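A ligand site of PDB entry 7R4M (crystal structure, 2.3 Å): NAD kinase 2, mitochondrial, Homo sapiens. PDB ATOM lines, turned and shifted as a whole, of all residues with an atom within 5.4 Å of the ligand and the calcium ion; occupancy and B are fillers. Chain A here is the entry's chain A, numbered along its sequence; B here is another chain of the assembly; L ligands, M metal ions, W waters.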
ATOM      1  N   GLY A 109      24.138 -13.126  25.560  1.00  0.00           N
ATOM      2  CA  GLY A 109      23.734 -14.006  24.475  1.00  0.00           C
ATOM      3  C   GLY A 109      24.011 -15.443  24.846  1.00  0.00           C
ATOM      4  O   GLY A 109      24.214 -15.754  26.018  1.00  0.00           O
ATOM      5  N   ASP A 110      24.036 -16.339  23.859  1.00  0.00           N
ATOM      6  CA  ASP A 110      24.288 -17.746  24.167  1.00  0.00           C
ATOM      7  C   ASP A 110      25.674 -17.920  24.808  1.00  0.00           C
ATOM      8  O   ASP A 110      25.836 -18.739  25.738  1.00  0.00           O
ATOM      9  CB  ASP A 110      24.127 -18.595  22.913  1.00  0.00           C
ATOM     10  CG  ASP A 110      22.672 -18.734  22.477  1.00  0.00           C
ATOM     11  OD1 ASP A 110      21.755 -18.554  23.327  1.00  0.00           O
ATOM     12  OD2 ASP A 110      22.428 -18.968  21.271  1.00  0.00           O
ATOM     13  N   GLY A 111      26.654 -17.144  24.358  1.00  0.00           N
ATOM     14  CA  GLY A 111      27.947 -17.154  25.033  1.00  0.00           C
ATOM     15  C   GLY A 111      27.838 -16.900  26.530  1.00  0.00           C
ATOM     16  O   GLY A 111      28.566 -17.501  27.341  1.00  0.00           O
ATOM     17  N   LEU A 114      26.500 -20.050  28.200  1.00  0.00           N
ATOM     18  CA  LEU A 114      27.534 -21.064  28.369  1.00  0.00           C
ATOM     19  C   LEU A 114      28.449 -20.723  29.548  1.00  0.00           C
ATOM     20  O   LEU A 114      28.845 -21.607  30.326  1.00  0.00           O
ATOM     21  CB  LEU A 114      28.345 -21.209  27.076  1.00  0.00           C
ATOM     22  CG  LEU A 114      27.574 -21.553  25.782  1.00  0.00           C
ATOM     23  CD1 LEU A 114      28.465 -21.375  24.521  1.00  0.00           C
ATOM     24  CD2 LEU A 114      26.986 -22.977  25.868  1.00  0.00           C
ATOM     25  N   ARG A 136      21.729  -8.380  17.596  1.00  0.00           N
ATOM     26  CA  ARG A 136      23.053  -8.937  17.352  1.00  0.00           C
ATOM     27  C   ARG A 136      23.302 -10.272  18.038  1.00  0.00           C
ATOM     28  O   ARG A 136      24.243 -10.980  17.645  1.00  0.00           O
ATOM     29  CB  ARG A 136      24.144  -7.938  17.778  1.00  0.00           C
ATOM     30  CG  ARG A 136      24.070  -6.624  17.028  1.00  0.00           C
ATOM     31  CD  ARG A 136      24.462  -6.804  15.575  1.00  0.00           C
ATOM     32  NE  ARG A 136      23.931  -5.745  14.716  1.00  0.00           N
ATOM     33  CZ  ARG A 136      24.678  -4.814  14.150  1.00  0.00           C
ATOM     34  NH1 ARG A 136      25.986  -4.756  14.335  1.00  0.00           N
ATOM     35  NH2 ARG A 136      24.093  -3.905  13.365  1.00  0.00           N
ATOM     36  N   SER A 137      22.502 -10.659  19.031  1.00  0.00           N
ATOM     37  CA  SER A 137      22.638 -11.935  19.704  1.00  0.00           C
ATOM     38  C   SER A 137      21.515 -12.863  19.255  1.00  0.00           C
ATOM     39  O   SER A 137      20.332 -12.504  19.321  1.00  0.00           O
ATOM     40  CB  SER A 137      22.598 -11.755  21.217  1.00  0.00           C
ATOM     41  OG  SER A 137      23.744 -11.066  21.670  1.00  0.00           O
ATOM     42  N   GLU A 138      21.896 -14.060  18.788  1.00  0.00           N
ATOM     43  CA  GLU A 138      20.917 -15.083  18.450  1.00  0.00           C
ATOM     44  C   GLU A 138      20.095 -15.502  19.674  1.00  0.00           C
ATOM     45  O   GLU A 138      18.855 -15.560  19.613  1.00  0.00           O
ATOM     46  CB  GLU A 138      21.626 -16.300  17.854  1.00  0.00           C
ATOM     47  CG  GLU A 138      20.840 -17.592  17.966  1.00  0.00           C
ATOM     48  CD  GLU A 138      20.046 -17.898  16.711  1.00  0.00           C
ATOM     49  OE1 GLU A 138      19.905 -16.990  15.863  1.00  0.00           O
ATOM     50  OE2 GLU A 138      19.573 -19.047  16.577  1.00  0.00           O
ATOM     51  N   GLY A 139      20.759 -15.790  20.793  1.00  0.00           N
ATOM     52  CA  GLY A 139      20.082 -16.118  22.034  1.00  0.00           C
ATOM     53  C   GLY A 139      19.167 -17.334  21.970  1.00  0.00           C
ATOM     54  O   GLY A 139      18.034 -17.312  22.465  1.00  0.00           O
ATOM     55  N   HIS A 140      19.672 -18.398  21.346  1.00  0.00           N
ATOM     56  CA  HIS A 140      18.903 -19.633  21.216  1.00  0.00           C
ATOM     57  C   HIS A 140      18.671 -20.290  22.571  1.00  0.00           C
ATOM     58  O   HIS A 140      17.623 -20.900  22.794  1.00  0.00           O
ATOM     59  CB  HIS A 140      19.656 -20.582  20.260  1.00  0.00           C
ATOM     60  CG  HIS A 140      18.850 -21.761  19.820  1.00  0.00           C
ATOM     61  ND1 HIS A 140      17.875 -21.670  18.849  1.00  0.00           N
ATOM     62  CD2 HIS A 140      18.867 -23.051  20.222  1.00  0.00           C
ATOM     63  CE1 HIS A 140      17.318 -22.855  18.671  1.00  0.00           C
ATOM     64  NE2 HIS A 140      17.901 -23.714  19.497  1.00  0.00           N
ATOM     65  N   LEU A 141      19.630 -20.162  23.494  1.00  0.00           N
ATOM     66  CA  LEU A 141      19.551 -20.727  24.832  1.00  0.00           C
ATOM     67  C   LEU A 141      18.832 -19.806  25.815  1.00  0.00           C
ATOM     68  O   LEU A 141      18.808 -20.093  27.015  1.00  0.00           O
ATOM     69  CB  LEU A 141      20.975 -21.052  25.337  1.00  0.00           C
ATOM     70  CG  LEU A 141      21.825 -21.986  24.459  1.00  0.00           C
ATOM     71  CD1 LEU A 141      23.165 -22.348  25.092  1.00  0.00           C
ATOM     72  CD2 LEU A 141      21.057 -23.240  24.135  1.00  0.00           C
ATOM     73  N   HIS A 188      38.810 -16.955  27.711  1.00  0.00           N
ATOM     74  CA  HIS A 188      38.487 -15.533  27.685  1.00  0.00           C
ATOM     75  C   HIS A 188      39.364 -14.731  28.628  1.00  0.00           C
ATOM     76  O   HIS A 188      38.980 -13.636  29.049  1.00  0.00           O
ATOM     77  CB  HIS A 188      36.988 -15.343  27.959  1.00  0.00           C
ATOM     78  CG  HIS A 188      36.129 -16.083  26.988  1.00  0.00           C
ATOM     79  ND1 HIS A 188      34.902 -16.623  27.317  1.00  0.00           N
ATOM     80  CD2 HIS A 188      36.342 -16.417  25.688  1.00  0.00           C
ATOM     81  CE1 HIS A 188      34.394 -17.237  26.271  1.00  0.00           C
ATOM     82  NE2 HIS A 188      35.246 -17.131  25.264  1.00  0.00           N
ATOM     83  N   ASN A 225      27.444 -27.290  25.080  1.00  0.00           N
ATOM     84  CA  ASN A 225      27.371 -27.355  23.624  1.00  0.00           C
ATOM     85  C   ASN A 225      28.148 -28.554  23.090  1.00  0.00           C
ATOM     86  O   ASN A 225      27.543 -29.488  22.553  1.00  0.00           O
ATOM     87  CB  ASN A 225      27.903 -26.072  22.964  1.00  0.00           C
ATOM     88  CG  ASN A 225      26.823 -25.039  22.787  1.00  0.00           C
ATOM     89  OD1 ASN A 225      25.650 -25.284  23.115  1.00  0.00           O
ATOM     90  ND2 ASN A 225      27.200 -23.873  22.264  1.00  0.00           N
ATOM     91  N   GLU A 226      29.472 -28.550  23.221  1.00  0.00           N
ATOM     92  CA  GLU A 226      30.293 -29.609  22.648  1.00  0.00           C
ATOM     93  C   GLU A 226      31.683 -29.587  23.268  1.00  0.00           C
ATOM     94  O   GLU A 226      32.118 -28.600  23.852  1.00  0.00           O
ATOM     95  CB  GLU A 226      30.452 -29.445  21.128  1.00  0.00           C
ATOM     96  CG  GLU A 226      31.443 -28.325  20.765  1.00  0.00           C
ATOM     97  CD  GLU A 226      30.796 -26.928  20.785  1.00  0.00           C
ATOM     98  OE1 GLU A 226      29.759 -26.761  20.104  1.00  0.00           O
ATOM     99  OE2 GLU A 226      31.322 -26.015  21.481  1.00  0.00           O
ATOM    100  N   THR A 263      21.652 -29.914  22.804  1.00  0.00           N
ATOM    101  CA  THR A 263      21.757 -28.456  22.819  1.00  0.00           C
ATOM    102  C   THR A 263      22.795 -27.990  21.810  1.00  0.00           C
ATOM    103  O   THR A 263      22.565 -27.055  21.038  1.00  0.00           O
ATOM    104  CB  THR A 263      22.107 -27.943  24.223  1.00  0.00           C
ATOM    105  OG1 THR A 263      21.021 -28.135  25.124  1.00  0.00           O
ATOM    106  CG2 THR A 263      22.409 -26.450  24.180  1.00  0.00           C
ATOM    107  N   GLY A 264      23.950 -28.639  21.797  1.00  0.00           N
ATOM    108  CA  GLY A 264      25.007 -28.258  20.872  1.00  0.00           C
ATOM    109  C   GLY A 264      24.774 -28.672  19.427  1.00  0.00           C
ATOM    110  O   GLY A 264      25.602 -28.325  18.573  1.00  0.00           O
ATOM    111  N   LYS A 266      22.665 -27.692  17.221  1.00  0.00           N
ATOM    112  CA  LYS A 266      22.393 -26.506  16.411  1.00  0.00           C
ATOM    113  C   LYS A 266      23.585 -25.547  16.318  1.00  0.00           C
ATOM    114  O   LYS A 266      23.547 -24.611  15.521  1.00  0.00           O
ATOM    115  CB  LYS A 266      21.176 -25.741  16.989  1.00  0.00           C
ATOM    116  CG  LYS A 266      19.896 -26.580  17.105  1.00  0.00           C
ATOM    117  CD  LYS A 266      19.827 -27.399  18.436  1.00  0.00           C
ATOM    118  CE  LYS A 266      18.416 -27.867  18.721  1.00  0.00           C
ATOM    119  NZ  LYS A 266      18.392 -29.274  19.229  1.00  0.00           N
ATOM    120  N   ALA A 267      24.624 -25.744  17.139  1.00  0.00           N
ATOM    121  CA  ALA A 267      25.784 -24.861  17.150  1.00  0.00           C
ATOM    122  C   ALA A 267      26.867 -25.343  16.162  1.00  0.00           C
ATOM    123  O   ALA A 267      26.553 -25.673  14.999  1.00  0.00           O
ATOM    124  CB  ALA A 267      26.328 -24.769  18.576  1.00  0.00           C
ATOM    125  N   TRP A 268      28.119 -25.383  16.604  1.00  0.00           N
ATOM    126  CA  TRP A 268      29.224 -25.755  15.707  1.00  0.00           C
ATOM    127  C   TRP A 268      28.906 -27.000  14.894  1.00  0.00           C
ATOM    128  O   TRP A 268      29.059 -27.012  13.661  1.00  0.00           O
ATOM    129  CB  TRP A 268      30.496 -25.981  16.522  1.00  0.00           C
ATOM    130  CG  TRP A 268      31.752 -25.747  15.763  1.00  0.00           C
ATOM    131  CD1 TRP A 268      31.883 -25.517  14.413  1.00  0.00           C
ATOM    132  CD2 TRP A 268      33.070 -25.696  16.304  1.00  0.00           C
ATOM    133  NE1 TRP A 268      33.203 -25.344  14.091  1.00  0.00           N
ATOM    134  CE2 TRP A 268      33.956 -25.454  15.235  1.00  0.00           C
ATOM    135  CE3 TRP A 268      33.597 -25.851  17.595  1.00  0.00           C
ATOM    136  CZ2 TRP A 268      35.343 -25.352  15.415  1.00  0.00           C
ATOM    137  CZ3 TRP A 268      34.953 -25.769  17.778  1.00  0.00           C
ATOM    138  CH2 TRP A 268      35.824 -25.507  16.689  1.00  0.00           C
ATOM    139  N   ASN A 271      27.100 -26.538  11.600  1.00  0.00           N
ATOM    140  CA  ASN A 271      27.791 -25.935  10.468  1.00  0.00           C
ATOM    141  C   ASN A 271      28.899 -26.814   9.943  1.00  0.00           C
ATOM    142  O   ASN A 271      29.310 -26.648   8.785  1.00  0.00           O
ATOM    143  CB  ASN A 271      28.308 -24.546  10.880  1.00  0.00           C
ATOM    144  CG  ASN A 271      27.181 -23.658  11.397  1.00  0.00           C
ATOM    145  OD1 ASN A 271      26.145 -23.507  10.750  1.00  0.00           O
ATOM    146  ND2 ASN A 271      27.354 -23.112  12.605  1.00  0.00           N
ATOM    147  N   ASP A 361      32.827 -25.922  25.141  1.00  0.00           N
ATOM    148  CA  ASP A 361      31.925 -24.794  24.855  1.00  0.00           C
ATOM    149  C   ASP A 361      32.665 -23.523  24.461  1.00  0.00           C
ATOM    150  O   ASP A 361      32.198 -22.409  24.751  1.00  0.00           O
ATOM    151  CB  ASP A 361      31.000 -24.500  26.038  1.00  0.00           C
ATOM    152  CG  ASP A 361      30.118 -25.688  26.413  1.00  0.00           C
ATOM    153  OD1 ASP A 361      30.061 -26.671  25.598  1.00  0.00           O
ATOM    154  OD2 ASP A 361      29.480 -25.645  27.518  1.00  0.00           O
ATOM    155  N   GLY A 362      33.814 -23.658  23.784  1.00  0.00           N
ATOM    156  CA  GLY A 362      34.577 -22.501  23.357  1.00  0.00           C
ATOM    157  C   GLY A 362      35.161 -21.646  24.483  1.00  0.00           C
ATOM    158  O   GLY A 362      35.649 -20.540  24.229  1.00  0.00           O
ATOM    159  N   SER B 234      41.387 -22.211  17.610  1.00  0.00           N
ATOM    160  CA  SER B 234      40.584 -23.090  16.776  1.00  0.00           C
ATOM    161  C   SER B 234      39.086 -22.919  17.027  1.00  0.00           C
ATOM    162  O   SER B 234      38.276 -23.166  16.126  1.00  0.00           O
ATOM    163  CB  SER B 234      41.021 -24.551  16.995  1.00  0.00           C
ATOM    164  OG  SER B 234      41.072 -24.892  18.371  1.00  0.00           O
ATOM    165  N   SER B 235      38.693 -22.521  18.232  1.00  0.00           N
ATOM    166  CA  SER B 235      37.279 -22.386  18.576  1.00  0.00           C
ATOM    167  C   SER B 235      36.752 -20.977  18.368  1.00  0.00           C
ATOM    168  O   SER B 235      35.569 -20.744  18.655  1.00  0.00           O
ATOM    169  CB  SER B 235      37.032 -22.800  20.035  1.00  0.00           C
ATOM    170  OG  SER B 235      37.790 -21.973  20.911  1.00  0.00           O
ATOM    171  N   ARG B 236      37.583 -20.042  17.927  1.00  0.00           N
ATOM    172  CA  ARG B 236      37.151 -18.663  17.735  1.00  0.00           C
ATOM    173  C   ARG B 236      36.632 -18.492  16.304  1.00  0.00           C
ATOM    174  O   ARG B 236      37.391 -18.647  15.335  1.00  0.00           O
ATOM    175  CB  ARG B 236      38.298 -17.680  18.021  1.00  0.00           C
ATOM    176  CG  ARG B 236      37.818 -16.265  18.129  1.00  0.00           C
ATOM    177  CD  ARG B 236      38.913 -15.203  18.299  1.00  0.00           C
ATOM    178  NE  ARG B 236      38.952 -14.722  19.678  1.00  0.00           N
ATOM    179  CZ  ARG B 236      39.942 -14.925  20.539  1.00  0.00           C
ATOM    180  NH1 ARG B 236      41.142 -15.359  20.152  1.00  0.00           N
ATOM    181  NH2 ARG B 236      39.750 -14.654  21.833  1.00  0.00           N
ATOM    182  N   ALA B 237      35.329 -18.222  16.176  1.00  0.00           N
ATOM    183  CA  ALA B 237      34.750 -17.861  14.890  1.00  0.00           C
ATOM    184  C   ALA B 237      35.535 -16.727  14.234  1.00  0.00           C
ATOM    185  O   ALA B 237      35.967 -15.784  14.913  1.00  0.00           O
ATOM    186  CB  ALA B 237      33.288 -17.435  15.077  1.00  0.00           C
ATOM    187  N   LYS B 253      30.802 -14.822   8.601  1.00  0.00           N
ATOM    188  CA  LYS B 253      31.274 -15.387   9.866  1.00  0.00           C
ATOM    189  C   LYS B 253      31.383 -16.888   9.673  1.00  0.00           C
ATOM    190  O   LYS B 253      30.413 -17.519   9.221  1.00  0.00           O
ATOM    191  CB  LYS B 253      30.334 -15.039  11.018  1.00  0.00           C
ATOM    192  CG  LYS B 253      30.942 -15.143  12.404  1.00  0.00           C
ATOM    193  CD  LYS B 253      30.118 -14.348  13.433  1.00  0.00           C
ATOM    194  CE  LYS B 253      30.914 -13.979  14.702  1.00  0.00           C
ATOM    195  NZ  LYS B 253      30.905 -12.513  15.018  1.00  0.00           N
ATOM    196  N   SER B 254      32.533 -17.469   9.994  1.00  0.00           N
ATOM    197  CA  SER B 254      32.765 -18.895   9.758  1.00  0.00           C
ATOM    198  C   SER B 254      34.011 -19.333  10.520  1.00  0.00           C
ATOM    199  O   SER B 254      34.599 -18.565  11.302  1.00  0.00           O
ATOM    200  CB  SER B 254      32.899 -19.160   8.262  1.00  0.00           C
ATOM    201  OG  SER B 254      34.114 -18.595   7.771  1.00  0.00           O
ATOM    202  N   SER B 255      34.435 -20.588  10.283  1.00  0.00           N
ATOM    203  CA  SER B 255      35.710 -21.088  10.762  1.00  0.00           C
ATOM    204  C   SER B 255      36.830 -20.926   9.732  1.00  0.00           C
ATOM    205  O   SER B 255      37.740 -21.762   9.672  1.00  0.00           O
ATOM    206  CB  SER B 255      35.600 -22.556  11.174  1.00  0.00           C
ATOM    207  OG  SER B 255      34.797 -22.744  12.324  1.00  0.00           O
ATOM    208  N   ARG B 327      34.577 -21.956   4.993  1.00  0.00           N
ATOM    209  CA  ARG B 327      34.643 -23.120   5.866  1.00  0.00           C
ATOM    210  C   ARG B 327      33.697 -22.971   7.053  1.00  0.00           C
ATOM    211  O   ARG B 327      33.866 -22.070   7.886  1.00  0.00           O
ATOM    212  CB  ARG B 327      36.080 -23.302   6.317  1.00  0.00           C
ATOM    213  CG  ARG B 327      36.323 -24.444   7.216  1.00  0.00           C
ATOM    214  CD  ARG B 327      37.728 -24.353   7.759  1.00  0.00           C
ATOM    215  NE  ARG B 327      38.156 -25.625   8.318  1.00  0.00           N
ATOM    216  CZ  ARG B 327      38.880 -25.749   9.409  1.00  0.00           C
ATOM    217  NH1 ARG B 327      39.278 -24.683  10.093  1.00  0.00           N
ATOM    218  NH2 ARG B 327      39.251 -26.978   9.813  1.00  0.00           N
ATOM    219  N   GLU B 328      32.715 -23.864   7.149  1.00  0.00           N
ATOM    220  CA  GLU B 328      31.719 -23.875   8.217  1.00  0.00           C
ATOM    221  C   GLU B 328      31.086 -22.496   8.499  1.00  0.00           C
ATOM    222  O   GLU B 328      31.223 -21.965   9.603  1.00  0.00           O
ATOM    223  CB  GLU B 328      32.320 -24.461   9.486  1.00  0.00           C
ATOM    224  CG  GLU B 328      32.904 -25.865   9.305  1.00  0.00           C
ATOM    225  CD  GLU B 328      33.933 -26.252  10.368  1.00  0.00           C
ATOM    226  OE1 GLU B 328      34.136 -25.435  11.315  1.00  0.00           O
ATOM    227  OE2 GLU B 328      34.516 -27.361  10.262  1.00  0.00           O
ATOM    228  N   PRO B 329      30.388 -21.919   7.523  1.00  0.00           N
ATOM    229  CA  PRO B 329      29.717 -20.630   7.780  1.00  0.00           C
ATOM    230  C   PRO B 329      28.603 -20.761   8.807  1.00  0.00           C
ATOM    231  O   PRO B 329      27.950 -21.803   8.924  1.00  0.00           O
ATOM    232  CB  PRO B 329      29.136 -20.256   6.403  1.00  0.00           C
ATOM    233  CG  PRO B 329      28.984 -21.541   5.707  1.00  0.00           C
ATOM    234  CD  PRO B 329      30.118 -22.404   6.161  1.00  0.00           C
ATOM    235  N   ILE B 330      28.413 -19.692   9.569  1.00  0.00           N
ATOM    236  CA  ILE B 330      27.321 -19.583  10.523  1.00  0.00           C
ATOM    237  C   ILE B 330      26.235 -18.718   9.901  1.00  0.00           C
ATOM    238  O   ILE B 330      26.487 -17.574   9.518  1.00  0.00           O
ATOM    239  CB  ILE B 330      27.805 -18.987  11.865  1.00  0.00           C
ATOM    240  CG1 ILE B 330      29.202 -19.509  12.213  1.00  0.00           C
ATOM    241  CG2 ILE B 330      26.807 -19.262  12.961  1.00  0.00           C
ATOM    242  CD1 ILE B 330      29.617 -19.210  13.626  1.00  0.00           C
ATOM    243  N   ASN B 332      22.111 -18.634  10.937  1.00  0.00           N
ATOM    244  CA  ASN B 332      21.049 -18.231  11.882  1.00  0.00           C
ATOM    245  C   ASN B 332      20.424 -16.837  11.682  1.00  0.00           C
ATOM    246  O   ASN B 332      20.477 -16.259  10.587  1.00  0.00           O
ATOM    247  CB  ASN B 332      21.476 -18.403  13.366  1.00  0.00           C
ATOM    248  CG  ASN B 332      22.677 -17.526  13.792  1.00  0.00           C
ATOM    249  OD1 ASN B 332      22.761 -16.344  13.476  1.00  0.00           O
ATOM    250  ND2 ASN B 332      23.569 -18.117  14.591  1.00  0.00           N
HETATM  251  P1  LIG L   1      30.040 -17.066  19.115  1.00  0.00           P
HETATM  252  O1  LIG L   1      29.256 -15.754  19.383  1.00  0.00           O
HETATM  253  O2  LIG L   1      31.049 -16.894  18.030  1.00  0.00           O
HETATM  254  O3  LIG L   1      28.973 -18.302  18.678  1.00  0.00           O
HETATM  255  C1  LIG L   1      28.539 -18.295  17.318  1.00  0.00           C
HETATM  256  C2  LIG L   1      27.001 -18.166  17.256  1.00  0.00           C
HETATM  257  O4  LIG L   1      26.347 -19.541  17.765  1.00  0.00           O
HETATM  258  C3  LIG L   1      26.540 -17.217  18.041  1.00  0.00           C
HETATM  259  O5  LIG L   1      25.525 -16.424  17.251  1.00  0.00           O
HETATM  260  C4  LIG L   1      25.815 -17.921  19.225  1.00  0.00           C
HETATM  261  O6  LIG L   1      24.662 -17.244  19.604  1.00  0.00           O
HETATM  262  C5  LIG L   1      25.352 -19.217  18.598  1.00  0.00           C
HETATM  263  N1  LIG L   1      25.196 -20.345  19.557  1.00  0.00           N
HETATM  264  C6  LIG L   1      25.950 -20.618  20.619  1.00  0.00           C
HETATM  265  N2  LIG L   1      25.531 -21.719  21.197  1.00  0.00           N
HETATM  266  C7  LIG L   1      24.451 -22.194  20.479  1.00  0.00           C
HETATM  267  C8  LIG L   1      23.566 -23.301  20.571  1.00  0.00           C
HETATM  268  N3  LIG L   1      23.687 -24.293  21.623  1.00  0.00           N
HETATM  269  N4  LIG L   1      22.606 -23.451  19.653  1.00  0.00           N
HETATM  270  C9  LIG L   1      22.473 -22.597  18.699  1.00  0.00           C
HETATM  271  N5  LIG L   1      23.271 -21.536  18.562  1.00  0.00           N
HETATM  272  C10 LIG L   1      24.267 -21.319  19.440  1.00  0.00           C
HETATM  273  O7  LIG L   1      30.818 -17.461  20.535  1.00  0.00           O
HETATM  274  P2  LIG L   1      29.983 -18.023  21.814  1.00  0.00           P
HETATM  275  O8  LIG L   1      28.664 -17.197  21.902  1.00  0.00           O
HETATM  276  O9  LIG L   1      30.833 -17.952  23.103  1.00  0.00           O
HETATM  277  O10 LIG L   1      29.539 -19.566  21.517  1.00  0.00           O
HETATM  278  C11 LIG L   1      30.488 -20.584  21.560  1.00  0.00           C
HETATM  279  C12 LIG L   1      29.924 -21.720  20.775  1.00  0.00           C
HETATM  280  O11 LIG L   1      29.934 -21.195  19.209  1.00  0.00           O
HETATM  281  C13 LIG L   1      30.716 -22.767  20.786  1.00  0.00           C
HETATM  282  O12 LIG L   1      30.380 -23.734  21.839  1.00  0.00           O
HETATM  283  C14 LIG L   1      30.511 -23.447  19.370  1.00  0.00           C
HETATM  284  O13 LIG L   1      29.551 -24.326  19.369  1.00  0.00           O
HETATM  285  C15 LIG L   1      30.091 -22.270  18.430  1.00  0.00           C
HETATM  286  N6  LIG L   1      31.091 -22.083  17.332  1.00  0.00           N
HETATM  287  C16 LIG L   1      30.694 -22.337  16.096  1.00  0.00           C
HETATM  288  C17 LIG L   1      31.597 -22.182  15.054  1.00  0.00           C
HETATM  289  C18 LIG L   1      31.083 -22.442  13.647  1.00  0.00           C
HETATM  290  O14 LIG L   1      29.877 -22.735  13.526  1.00  0.00           O
HETATM  291  N7  LIG L   1      31.961 -22.310  12.529  1.00  0.00           N
HETATM  292  C19 LIG L   1      32.923 -21.765  15.272  1.00  0.00           C
HETATM  293  C20 LIG L   1      33.278 -21.537  16.589  1.00  0.00           C
HETATM  294  C21 LIG L   1      32.326 -21.702  17.613  1.00  0.00           C
HETATM  295  P3  LIG L   1      24.743 -15.707  20.260  1.00  0.00           P
HETATM  296  O15 LIG L   1      23.518 -15.511  21.303  1.00  0.00           O
HETATM  297  O16 LIG L   1      24.635 -14.740  19.113  1.00  0.00           O
HETATM  298  O17 LIG L   1      26.058 -15.497  20.939  1.00  0.00           O
HETATM  299 CA    CA M   1      28.354 -14.897  21.361  1.00  0.00          CA
HETATM  300  O   HOH W   1      28.083 -12.632  20.626  1.00  0.00           O
HETATM  301  O   HOH W   2      31.968 -14.226  17.711  1.00  0.00           O
HETATM  302  O   HOH W   3      30.527 -14.125  22.201  1.00  0.00           O
HETATM  303  O   HOH W   4      33.736 -20.069  20.368  1.00  0.00           O
HETATM  304  O   HOH W   5      33.664 -18.114  18.455  1.00  0.00           O
HETATM  305  O   HOH W   6      27.393 -13.990  23.812  1.00  0.00           O
HETATM  306  O   HOH W   7      32.285 -19.894  25.243  1.00  0.00           O
HETATM  307  O   HOH W   8      27.420 -21.837  16.094  1.00  0.00           O
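The side-chain carboxylate (OE2) of Glu 226 is in hydrogen-bond range of an oxygen (O12) of the ligand (2.5 Å).
OD1 of Asn 225 is in hydrogen-bond range of N3 of the ligand, 2.7 Å away.
The side-chain amide nitrogen (ND2) of Asn 271 lies within hydrogen-bond range of an oxygen (O14) of the ligand.
The backbone NH (N) of Asp 110 is in hydrogen-bond range of an oxygen (O15) of the ligand (2.7 Å).
O15 of the ligand lies within hydrogen-bond range of N of Gly 139 (2.8 Å).
The backbone NH (N) of Glu 138 is in hydrogen-bond range of an oxygen (O16) of the ligand, at 2.8 Å.
A nitrogen (N7) of the ligand is in hydrogen-bond range of the side-chain hydroxyl of Ser 255 of chain B.
The backbone carbonyl oxygen (O) of Glu 328 of chain B lies within hydrogen-bond range of a nitrogen (N7) of the ligand (3.0 Å).
The backbone carbonyl oxygen (O) of Thr 263 sits at hydrogen-bond distance from a nitrogen (N3) of the ligand.
O8 of the ligand sits close to N of Gly 111, at 3.2 Å.
O13 of the ligand is in hydrogen-bond range of N of Trp 268 (3.3 Å).
The side-chain carboxylate of Asp 361 sits at hydrogen-bond distance from the backbone NH of Asn 225 (2.7 Å).
The side-chain amide oxygen (OD1) of Asn 271 sits close to the backbone carbonyl oxygen (O) of Pro 329 of chain B, 3.1 Å away.
OD1 of Asp 110 lies within hydrogen-bond range of N of Leu 141 (2.7 Å).
The side-chain carboxylate of Asp 110 lies within hydrogen-bond range of the backbone NH of His 140.
The side-chain hydroxyl (OG) of Ser 255 of chain B lies within hydrogen-bond range of the side-chain carboxylate (OE1) of Glu 328 of chain B, at 2.9 Å.
O of Arg 327 of chain B sits at hydrogen-bond distance from N of Ser 255 of chain B, 2.9 Å away.
The side-chain carboxylate (OE1) of Glu 328 of chain B sits at hydrogen-bond distance from the indole nitrogen (NE1) of Trp 268 (2.9 Å).
N of Ile 330 of chain B is in hydrogen-bond range of O of Lys 253 of chain B, at 3.0 Å.
CA of Gly 109 touches O15 of the ligand, at 3.5 Å.
Leu 114 touches the ligand.
CA of Ser 137 touches O16 of the ligand, 3.5 Å away.
CB of His 140 touches C9 of the ligand, at 3.8 Å.
CD2 of Leu 141 touches N3 of the ligand (3.8 Å).
Lys 266 touches the ligand.
Ala 267 touches the ligand.
Asp 361 touches the ligand (C to O12, 3.5 Å).
Gly 362 touches the ligand (N to O12, 3.9 Å).
Ser 235 of chain B touches the ligand.
Ala 237 of chain B touches the ligand (CB to O2, 3.7 Å).
CD1 of Ile 330 of chain B touches O14 of the ligand, 3.5 Å away.
ND2 of Asn 332 of chain B touches O5 of the ligand, at 3.7 Å.
24 residues have an atom within 4 Å of the ligand: Gly 109, Asp 110, Gly 111, Leu 114, Ser 137, Glu 138, Gly 139, His 140, Leu 141, Asn 225, Glu 226, Thr 263, Lys 266, Ala 267, Trp 268, Asn 271, Asp 361, Gly 362, Ser 235 of chain B, Ala 237 of chain B, Ser 255 of chain B, Glu 328 of chain B, Ile 330 of chain B and Asn 332 of chain B.
No residue comes within 4 Å of the calcium ion.
The nearest printed residue that does not touch the calcium ion is Gly 111 (4.1 Å).
The calcium ion is bound by O1 of the ligand, O8 of the ligand, water W1, O17 of the ligand, water W3 and water W6.
Water W2 lies within hydrogen-bond range of an oxygen (O2) of the ligand and the side-chain amino group of Lys 253 of chain B.
Water W5 lies within hydrogen-bond range of the backbone NH of Ala 237 of chain B, an oxygen (O2) of the ligand and the backbone carbonyl oxygen of Ser 235 of chain B.
Water W7 lies within hydrogen-bond range of O of Asp 361 (2.6 Å) and O9 of the ligand (3.2 Å).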
